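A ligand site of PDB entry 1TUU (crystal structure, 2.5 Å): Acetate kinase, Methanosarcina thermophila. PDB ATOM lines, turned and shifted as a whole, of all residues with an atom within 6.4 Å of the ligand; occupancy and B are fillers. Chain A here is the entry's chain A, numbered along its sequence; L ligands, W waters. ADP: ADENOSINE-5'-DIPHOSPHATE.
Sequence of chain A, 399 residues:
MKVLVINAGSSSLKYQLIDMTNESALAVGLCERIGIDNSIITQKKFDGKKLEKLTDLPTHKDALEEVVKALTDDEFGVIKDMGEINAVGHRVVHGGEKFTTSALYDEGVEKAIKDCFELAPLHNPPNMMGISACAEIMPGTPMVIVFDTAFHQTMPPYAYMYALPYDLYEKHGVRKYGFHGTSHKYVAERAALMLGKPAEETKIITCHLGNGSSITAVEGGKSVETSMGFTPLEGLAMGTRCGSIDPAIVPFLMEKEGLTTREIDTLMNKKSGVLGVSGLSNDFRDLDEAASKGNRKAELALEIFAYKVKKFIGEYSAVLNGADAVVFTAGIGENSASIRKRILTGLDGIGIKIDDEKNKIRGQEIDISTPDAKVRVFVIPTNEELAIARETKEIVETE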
ATOM      1  N   LYS A  14      11.419  -2.773 -38.648  1.00  0.00           N
ATOM      2  CA  LYS A  14      11.895  -3.338 -37.395  1.00  0.00           C
ATOM      3  C   LYS A  14      11.263  -4.697 -37.152  1.00  0.00           C
ATOM      4  O   LYS A  14      10.036  -4.811 -37.088  1.00  0.00           O
ATOM      5  CB  LYS A  14      11.531  -2.435 -36.213  1.00  0.00           C
ATOM      6  CG  LYS A  14      12.455  -1.264 -35.963  1.00  0.00           C
ATOM      7  CD  LYS A  14      11.847  -0.294 -34.932  1.00  0.00           C
ATOM      8  CE  LYS A  14      11.484  -1.025 -33.644  1.00  0.00           C
ATOM      9  NZ  LYS A  14      10.805  -0.129 -32.642  1.00  0.00           N
ATOM     10  N   LEU A  30      16.785  -4.718 -37.813  1.00  0.00           N
ATOM     11  CA  LEU A  30      16.211  -3.533 -38.415  1.00  0.00           C
ATOM     12  C   LEU A  30      16.677  -3.434 -39.852  1.00  0.00           C
ATOM     13  O   LEU A  30      17.823  -3.767 -40.179  1.00  0.00           O
ATOM     14  CB  LEU A  30      16.666  -2.274 -37.661  1.00  0.00           C
ATOM     15  CG  LEU A  30      16.322  -0.922 -38.298  1.00  0.00           C
ATOM     16  CD1 LEU A  30      14.966  -0.464 -37.784  1.00  0.00           C
ATOM     17  CD2 LEU A  30      17.378   0.098 -37.946  1.00  0.00           C
ATOM     18  N   HIS A 208       5.051   8.338 -24.103  1.00  0.00           N
ATOM     19  CA  HIS A 208       5.749   7.653 -25.181  1.00  0.00           C
ATOM     20  C   HIS A 208       6.360   8.788 -26.034  1.00  0.00           C
ATOM     21  O   HIS A 208       5.624   9.604 -26.588  1.00  0.00           O
ATOM     22  CB  HIS A 208       4.744   6.836 -25.994  1.00  0.00           C
ATOM     23  CG  HIS A 208       5.352   5.971 -27.069  1.00  0.00           C
ATOM     24  ND1 HIS A 208       5.708   4.655 -26.854  1.00  0.00           N
ATOM     25  CD2 HIS A 208       5.641   6.231 -28.366  1.00  0.00           C
ATOM     26  CE1 HIS A 208       6.171   4.135 -27.979  1.00  0.00           C
ATOM     27  NE2 HIS A 208       6.148   5.077 -28.908  1.00  0.00           N
ATOM     28  N   LEU A 209       7.691   8.890 -26.104  1.00  0.00           N
ATOM     29  CA  LEU A 209       8.287   9.958 -26.914  1.00  0.00           C
ATOM     30  C   LEU A 209       9.273   9.366 -27.933  1.00  0.00           C
ATOM     31  O   LEU A 209      10.372   8.934 -27.570  1.00  0.00           O
ATOM     32  CB  LEU A 209       8.996  10.979 -26.017  1.00  0.00           C
ATOM     33  CG  LEU A 209       8.259  11.438 -24.744  1.00  0.00           C
ATOM     34  CD1 LEU A 209       9.148  12.331 -23.897  1.00  0.00           C
ATOM     35  CD2 LEU A 209       6.978  12.155 -25.114  1.00  0.00           C
ATOM     36  N   GLY A 210       8.860   9.348 -29.196  1.00  0.00           N
ATOM     37  CA  GLY A 210       9.707   8.807 -30.245  1.00  0.00           C
ATOM     38  C   GLY A 210       9.438   9.599 -31.498  1.00  0.00           C
ATOM     39  O   GLY A 210       9.054  10.750 -31.393  1.00  0.00           O
ATOM     40  N   ASN A 211       9.613   9.002 -32.675  1.00  0.00           N
ATOM     41  CA  ASN A 211       9.334   9.730 -33.901  1.00  0.00           C
ATOM     42  C   ASN A 211       7.984  10.406 -33.708  1.00  0.00           C
ATOM     43  O   ASN A 211       7.745  11.529 -34.162  1.00  0.00           O
ATOM     44  CB  ASN A 211       9.250   8.793 -35.098  1.00  0.00           C
ATOM     45  CG  ASN A 211      10.303   9.080 -36.135  1.00  0.00           C
ATOM     46  OD1 ASN A 211      11.482   8.761 -35.937  1.00  0.00           O
ATOM     47  ND2 ASN A 211       9.901   9.708 -37.245  1.00  0.00           N
ATOM     48  N   GLY A 212       7.104   9.679 -33.040  1.00  0.00           N
ATOM     49  CA  GLY A 212       5.783  10.201 -32.745  1.00  0.00           C
ATOM     50  C   GLY A 212       5.729  10.183 -31.244  1.00  0.00           C
ATOM     51  O   GLY A 212       6.352   9.330 -30.624  1.00  0.00           O
ATOM     52  N   ASN A 282      14.502  15.777 -38.234  1.00  0.00           N
ATOM     53  CA  ASN A 282      13.461  15.271 -37.342  1.00  0.00           C
ATOM     54  C   ASN A 282      14.046  14.388 -36.259  1.00  0.00           C
ATOM     55  O   ASN A 282      13.321  13.917 -35.385  1.00  0.00           O
ATOM     56  CB  ASN A 282      12.470  14.437 -38.134  1.00  0.00           C
ATOM     57  CG  ASN A 282      13.116  13.222 -38.755  1.00  0.00           C
ATOM     58  OD1 ASN A 282      14.213  13.322 -39.290  1.00  0.00           O
ATOM     59  ND2 ASN A 282      12.443  12.087 -38.714  1.00  0.00           N
ATOM     60  N   ASP A 283      15.349  14.137 -36.331  1.00  0.00           N
ATOM     61  CA  ASP A 283      16.021  13.287 -35.357  1.00  0.00           C
ATOM     62  C   ASP A 283      16.340  14.105 -34.114  1.00  0.00           C
ATOM     63  O   ASP A 283      17.094  15.081 -34.165  1.00  0.00           O
ATOM     64  CB  ASP A 283      17.302  12.728 -35.977  1.00  0.00           C
ATOM     65  CG  ASP A 283      17.940  11.672 -35.131  1.00  0.00           C
ATOM     66  OD1 ASP A 283      17.299  10.629 -34.913  1.00  0.00           O
ATOM     67  OD2 ASP A 283      19.076  11.888 -34.685  1.00  0.00           O
ATOM     68  N   PHE A 284      15.783  13.705 -32.977  1.00  0.00           N
ATOM     69  CA  PHE A 284      16.010  14.440 -31.745  1.00  0.00           C
ATOM     70  C   PHE A 284      17.449  14.352 -31.258  1.00  0.00           C
ATOM     71  O   PHE A 284      17.928  15.232 -30.547  1.00  0.00           O
ATOM     72  CB  PHE A 284      15.021  13.997 -30.656  1.00  0.00           C
ATOM     73  CG  PHE A 284      13.602  14.494 -30.878  1.00  0.00           C
ATOM     74  CD1 PHE A 284      12.772  13.912 -31.832  1.00  0.00           C
ATOM     75  CD2 PHE A 284      13.111  15.552 -30.130  1.00  0.00           C
ATOM     76  CE1 PHE A 284      11.467  14.378 -32.023  1.00  0.00           C
ATOM     77  CE2 PHE A 284      11.814  16.030 -30.317  1.00  0.00           C
ATOM     78  CZ  PHE A 284      10.987  15.441 -31.259  1.00  0.00           C
ATOM     79  N   ARG A 285      18.140  13.295 -31.655  1.00  0.00           N
ATOM     80  CA  ARG A 285      19.533  13.141 -31.279  1.00  0.00           C
ATOM     81  C   ARG A 285      20.292  14.245 -31.988  1.00  0.00           C
ATOM     82  O   ARG A 285      21.056  14.978 -31.371  1.00  0.00           O
ATOM     83  CB  ARG A 285      20.041  11.775 -31.709  1.00  0.00           C
ATOM     84  CG  ARG A 285      21.076  11.183 -30.788  1.00  0.00           C
ATOM     85  CD  ARG A 285      21.645   9.900 -31.360  1.00  0.00           C
ATOM     86  NE  ARG A 285      20.590   8.963 -31.776  1.00  0.00           N
ATOM     87  CZ  ARG A 285      20.168   8.812 -33.031  1.00  0.00           C
ATOM     88  NH1 ARG A 285      20.697   9.546 -34.009  1.00  0.00           N
ATOM     89  NH2 ARG A 285      19.214   7.917 -33.304  1.00  0.00           N
ATOM     90  N   ASP A 286      20.069  14.355 -33.296  1.00  0.00           N
ATOM     91  CA  ASP A 286      20.744  15.386 -34.062  1.00  0.00           C
ATOM     92  C   ASP A 286      20.454  16.735 -33.466  1.00  0.00           C
ATOM     93  O   ASP A 286      21.357  17.547 -33.272  1.00  0.00           O
ATOM     94  CB  ASP A 286      20.286  15.370 -35.508  1.00  0.00           C
ATOM     95  CG  ASP A 286      20.675  14.104 -36.223  1.00  0.00           C
ATOM     96  OD1 ASP A 286      21.537  13.375 -35.694  1.00  0.00           O
ATOM     97  OD2 ASP A 286      20.117  13.825 -37.307  1.00  0.00           O
ATOM     98  N   ASP A 288      19.549  17.500 -30.444  1.00  0.00           N
ATOM     99  CA  ASP A 288      20.165  17.653 -29.137  1.00  0.00           C
ATOM    100  C   ASP A 288      21.595  18.151 -29.307  1.00  0.00           C
ATOM    101  O   ASP A 288      21.989  19.140 -28.708  1.00  0.00           O
ATOM    102  CB  ASP A 288      20.163  16.318 -28.402  1.00  0.00           C
ATOM    103  CG  ASP A 288      20.587  16.450 -26.954  1.00  0.00           C
ATOM    104  OD1 ASP A 288      20.956  17.578 -26.554  1.00  0.00           O
ATOM    105  OD2 ASP A 288      20.581  15.440 -26.223  1.00  0.00           O
ATOM    106  N   ALA A 330      10.085   4.924 -24.837  1.00  0.00           N
ATOM    107  CA  ALA A 330      10.340   5.116 -26.266  1.00  0.00           C
ATOM    108  C   ALA A 330      11.724   5.707 -26.532  1.00  0.00           C
ATOM    109  O   ALA A 330      12.504   5.927 -25.611  1.00  0.00           O
ATOM    110  CB  ALA A 330       9.268   5.988 -26.891  1.00  0.00           C
ATOM    111  N   GLY A 331      12.019   5.955 -27.805  1.00  0.00           N
ATOM    112  CA  GLY A 331      13.322   6.490 -28.185  1.00  0.00           C
ATOM    113  C   GLY A 331      13.844   7.633 -27.344  1.00  0.00           C
ATOM    114  O   GLY A 331      14.871   7.505 -26.681  1.00  0.00           O
ATOM    115  N   ILE A 332      13.125   8.755 -27.336  1.00  0.00           N
ATOM    116  CA  ILE A 332      13.512   9.935 -26.574  1.00  0.00           C
ATOM    117  C   ILE A 332      13.348   9.705 -25.072  1.00  0.00           C
ATOM    118  O   ILE A 332      14.246   9.992 -24.291  1.00  0.00           O
ATOM    119  CB  ILE A 332      12.652  11.153 -26.985  1.00  0.00           C
ATOM    120  CG1 ILE A 332      12.640  11.290 -28.500  1.00  0.00           C
ATOM    121  CG2 ILE A 332      13.215  12.408 -26.356  1.00  0.00           C
ATOM    122  CD1 ILE A 332      11.728  12.380 -29.013  1.00  0.00           C
ATOM    123  N   GLY A 333      12.186   9.196 -24.671  1.00  0.00           N
ATOM    124  CA  GLY A 333      11.918   8.984 -23.265  1.00  0.00           C
ATOM    125  C   GLY A 333      12.831   8.059 -22.500  1.00  0.00           C
ATOM    126  O   GLY A 333      13.024   8.217 -21.300  1.00  0.00           O
ATOM    127  N   GLU A 334      13.394   7.076 -23.195  1.00  0.00           N
ATOM    128  CA  GLU A 334      14.275   6.090 -22.566  1.00  0.00           C
ATOM    129  C   GLU A 334      15.730   6.548 -22.527  1.00  0.00           C
ATOM    130  O   GLU A 334      16.400   6.459 -21.500  1.00  0.00           O
ATOM    131  CB  GLU A 334      14.232   4.766 -23.337  1.00  0.00           C
ATOM    132  CG  GLU A 334      12.946   3.974 -23.244  1.00  0.00           C
ATOM    133  CD  GLU A 334      12.868   2.882 -24.311  1.00  0.00           C
ATOM    134  OE1 GLU A 334      13.926   2.301 -24.629  1.00  0.00           O
ATOM    135  OE2 GLU A 334      11.761   2.631 -24.830  1.00  0.00           O
ATOM    136  N   ASN A 335      16.194   7.056 -23.669  1.00  0.00           N
ATOM    137  CA  ASN A 335      17.585   7.455 -23.782  1.00  0.00           C
ATOM    138  C   ASN A 335      17.925   8.897 -23.467  1.00  0.00           C
ATOM    139  O   ASN A 335      18.903   9.161 -22.798  1.00  0.00           O
ATOM    140  CB  ASN A 335      18.069   7.121 -25.191  1.00  0.00           C
ATOM    141  CG  ASN A 335      17.536   5.790 -25.655  1.00  0.00           C
ATOM    142  OD1 ASN A 335      17.773   4.753 -25.036  1.00  0.00           O
ATOM    143  ND2 ASN A 335      16.802   5.814 -26.755  1.00  0.00           N
ATOM    144  N   SER A 336      17.117   9.839 -23.933  1.00  0.00           N
ATOM    145  CA  SER A 336      17.442  11.236 -23.670  1.00  0.00           C
ATOM    146  C   SER A 336      17.241  11.661 -22.210  1.00  0.00           C
ATOM    147  O   SER A 336      16.132  11.639 -21.690  1.00  0.00           O
ATOM    148  CB  SER A 336      16.638  12.157 -24.585  1.00  0.00           C
ATOM    149  OG  SER A 336      17.012  13.504 -24.367  1.00  0.00           O
ATOM    150  N   ALA A 337      18.345  12.042 -21.576  1.00  0.00           N
ATOM    151  CA  ALA A 337      18.356  12.489 -20.195  1.00  0.00           C
ATOM    152  C   ALA A 337      18.220  14.018 -20.201  1.00  0.00           C
ATOM    153  O   ALA A 337      17.605  14.603 -19.315  1.00  0.00           O
ATOM    154  CB  ALA A 337      19.666  12.101 -19.529  1.00  0.00           C
ATOM    155  N   SER A 338      18.809  14.631 -21.222  1.00  0.00           N
ATOM    156  CA  SER A 338      18.765  16.071 -21.392  1.00  0.00           C
ATOM    157  C   SER A 338      17.339  16.550 -21.678  1.00  0.00           C
ATOM    158  O   SER A 338      16.858  17.450 -21.004  1.00  0.00           O
ATOM    159  CB  SER A 338      19.718  16.492 -22.524  1.00  0.00           C
ATOM    160  OG  SER A 338      19.295  15.998 -23.790  1.00  0.00           O
ATOM    161  N   ILE A 339      16.685  15.945 -22.661  1.00  0.00           N
ATOM    162  CA  ILE A 339      15.327  16.343 -22.996  1.00  0.00           C
ATOM    163  C   ILE A 339      14.431  16.068 -21.796  1.00  0.00           C
ATOM    164  O   ILE A 339      13.573  16.882 -21.448  1.00  0.00           O
ATOM    165  CB  ILE A 339      14.837  15.578 -24.261  1.00  0.00           C
ATOM    166  CG1 ILE A 339      15.535  16.178 -25.493  1.00  0.00           C
ATOM    167  CG2 ILE A 339      13.313  15.632 -24.389  1.00  0.00           C
ATOM    168  CD1 ILE A 339      15.527  15.316 -26.727  1.00  0.00           C
ATOM    169  N   THR A 382      10.322   0.622 -23.314  1.00  0.00           N
ATOM    170  CA  THR A 382       9.134  -0.019 -23.825  1.00  0.00           C
ATOM    171  C   THR A 382       9.453  -1.312 -24.545  1.00  0.00           C
ATOM    172  O   THR A 382      10.572  -1.514 -25.019  1.00  0.00           O
ATOM    173  CB  THR A 382       8.418   0.874 -24.832  1.00  0.00           C
ATOM    174  OG1 THR A 382       7.148   0.302 -25.142  1.00  0.00           O
ATOM    175  CG2 THR A 382       9.244   0.991 -26.111  1.00  0.00           C
ATOM    176  N   GLU A 384       6.983  -3.121 -27.016  1.00  0.00           N
ATOM    177  CA  GLU A 384       5.786  -3.421 -27.797  1.00  0.00           C
ATOM    178  C   GLU A 384       5.843  -4.824 -28.389  1.00  0.00           C
ATOM    179  O   GLU A 384       4.844  -5.548 -28.379  1.00  0.00           O
ATOM    180  CB  GLU A 384       5.651  -2.421 -28.928  1.00  0.00           C
ATOM    181  CG  GLU A 384       5.564  -1.002 -28.483  1.00  0.00           C
ATOM    182  CD  GLU A 384       5.587  -0.061 -29.658  1.00  0.00           C
ATOM    183  OE1 GLU A 384       4.793  -0.279 -30.607  1.00  0.00           O
ATOM    184  OE2 GLU A 384       6.409   0.891 -29.649  1.00  0.00           O
HETATM  185  PB  ADP L   1      13.106   3.448 -32.348  1.00  0.00           P
HETATM  186  O1B ADP L   1      14.401   3.984 -32.912  1.00  0.00           O
HETATM  187  O2B ADP L   1      12.615   2.154 -32.965  1.00  0.00           O
HETATM  188  O3B ADP L   1      13.178   3.351 -30.787  1.00  0.00           O
HETATM  189  PA  ADP L   1      11.308   5.690 -31.664  1.00  0.00           P
HETATM  190  O1A ADP L   1      10.888   5.119 -30.346  1.00  0.00           O
HETATM  191  O2A ADP L   1      10.302   6.365 -32.453  1.00  0.00           O
HETATM  192  O3A ADP L   1      11.968   4.506 -32.580  1.00  0.00           O
HETATM  193  O5' ADP L   1      12.586   6.584 -31.379  1.00  0.00           O
HETATM  194  C5' ADP L   1      13.278   7.244 -32.474  1.00  0.00           C
HETATM  195  C4' ADP L   1      13.780   8.637 -32.158  1.00  0.00           C
HETATM  196  O4' ADP L   1      13.993   8.738 -30.716  1.00  0.00           O
HETATM  197  C3' ADP L   1      15.158   9.092 -32.694  1.00  0.00           C
HETATM  198  O3' ADP L   1      14.997   9.461 -34.072  1.00  0.00           O
HETATM  199  C2' ADP L   1      15.409  10.380 -31.755  1.00  0.00           C
HETATM  200  O2' ADP L   1      14.600  11.512 -32.215  1.00  0.00           O
HETATM  201  C1' ADP L   1      14.919   9.805 -30.374  1.00  0.00           C
HETATM  202  N9  ADP L   1      16.106   9.272 -29.566  1.00  0.00           N
HETATM  203  C8  ADP L   1      16.411   8.012 -29.294  1.00  0.00           C
HETATM  204  N7  ADP L   1      17.495   7.915 -28.605  1.00  0.00           N
HETATM  205  C5  ADP L   1      17.917   9.221 -28.395  1.00  0.00           C
HETATM  206  C6  ADP L   1      19.045   9.841 -27.711  1.00  0.00           C
HETATM  207  N6  ADP L   1      20.018   9.129 -27.039  1.00  0.00           N
HETATM  208  N1  ADP L   1      19.127  11.198 -27.718  1.00  0.00           N
HETATM  209  C2  ADP L   1      18.205  11.909 -28.362  1.00  0.00           C
HETATM  210  N3  ADP L   1      17.146  11.430 -29.024  1.00  0.00           N
HETATM  211  C4  ADP L   1      17.048  10.067 -28.992  1.00  0.00           C
HETATM  212  O   HOH W   1       7.273   5.655 -31.062  1.00  0.00           O
HETATM  213  O   HOH W   2      20.259   6.077 -28.578  1.00  0.00           O
HETATM  214  O   HOH W   3      19.598  13.221 -25.895  1.00  0.00           O
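Water W3 lies within hydrogen-bond range of the side-chain carboxylate (OD2) of Asp 288 (2.4 Å), a nitrogen (N1) of the ligand (2.8 Å), the side-chain hydroxyl (OG) of Ser 336 (3.0 Å) and the side-chain hydroxyl (OG) of Ser 338 (3.5 Å). Water W1 lies within hydrogen-bond range of a ring nitrogen (NE2) of His 208 (2.5 Å) and an oxygen (O2A) of the ligand (3.4 Å).
NH1 of Arg 285 lies within salt-bridge range of OD2 of Asp 283. The side-chain carboxylate of Asp 283 is in hydrogen-bond range of the backbone NH of Asp 286 (3.0 Å). The backbone carbonyl oxygen of Gly 331 sits at hydrogen-bond distance from the side-chain amide nitrogen of Asn 335 (2.6 Å). N of Gly 331 sits at hydrogen-bond distance from O of Leu 209 (3.4 Å). O of Leu 209 lies within hydrogen-bond range of N of Ile 332 (2.8 Å). N of Ala 330 lies within hydrogen-bond range of OE2 of Glu 334, 2.8 Å away.
N of Phe 284 sits at hydrogen-bond distance from O2' of the ligand. The side-chain carboxylate of Asp 283 sits at hydrogen-bond distance from an oxygen (O3') of the ligand (2.7 Å). The backbone NH of Asn 211 is in hydrogen-bond range of an oxygen (O2A) of the ligand (2.7 Å). ND2 of Asn 335 sits at hydrogen-bond distance from N7 of the ligand (2.9 Å). N of Gly 331 lies within hydrogen-bond range of O1A of the ligand (2.9 Å). NZ of Lys 14 is in salt-bridge range of O2B of the ligand, at 2.9 Å. An oxygen (O4') of the ligand is in hydrogen-bond range of the backbone NH (N) of Ile 332, at 3.5 Å. A nitrogen (N3) of the ligand lies within hydrogen-bond range of the backbone NH (N) of Arg 285.
CA of Gly 210 touches O2A of the ligand (3.3 Å). Ala 330 touches the ligand (CB to O1A, 3.9 Å). Hydrophobic or aromatic side chains within 4 Å of the ligand: Phe 284, Ala 330 and Ile 332. Within 4 Å of the ligand: Lys 14, Gly 210, Asn 211, Asp 283, Phe 284, Arg 285, Ala 330, Gly 331, Ile 332 and Asn 335. The nearest printed residue that does not touch the ligand is Ser 336 (4.1 Å).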
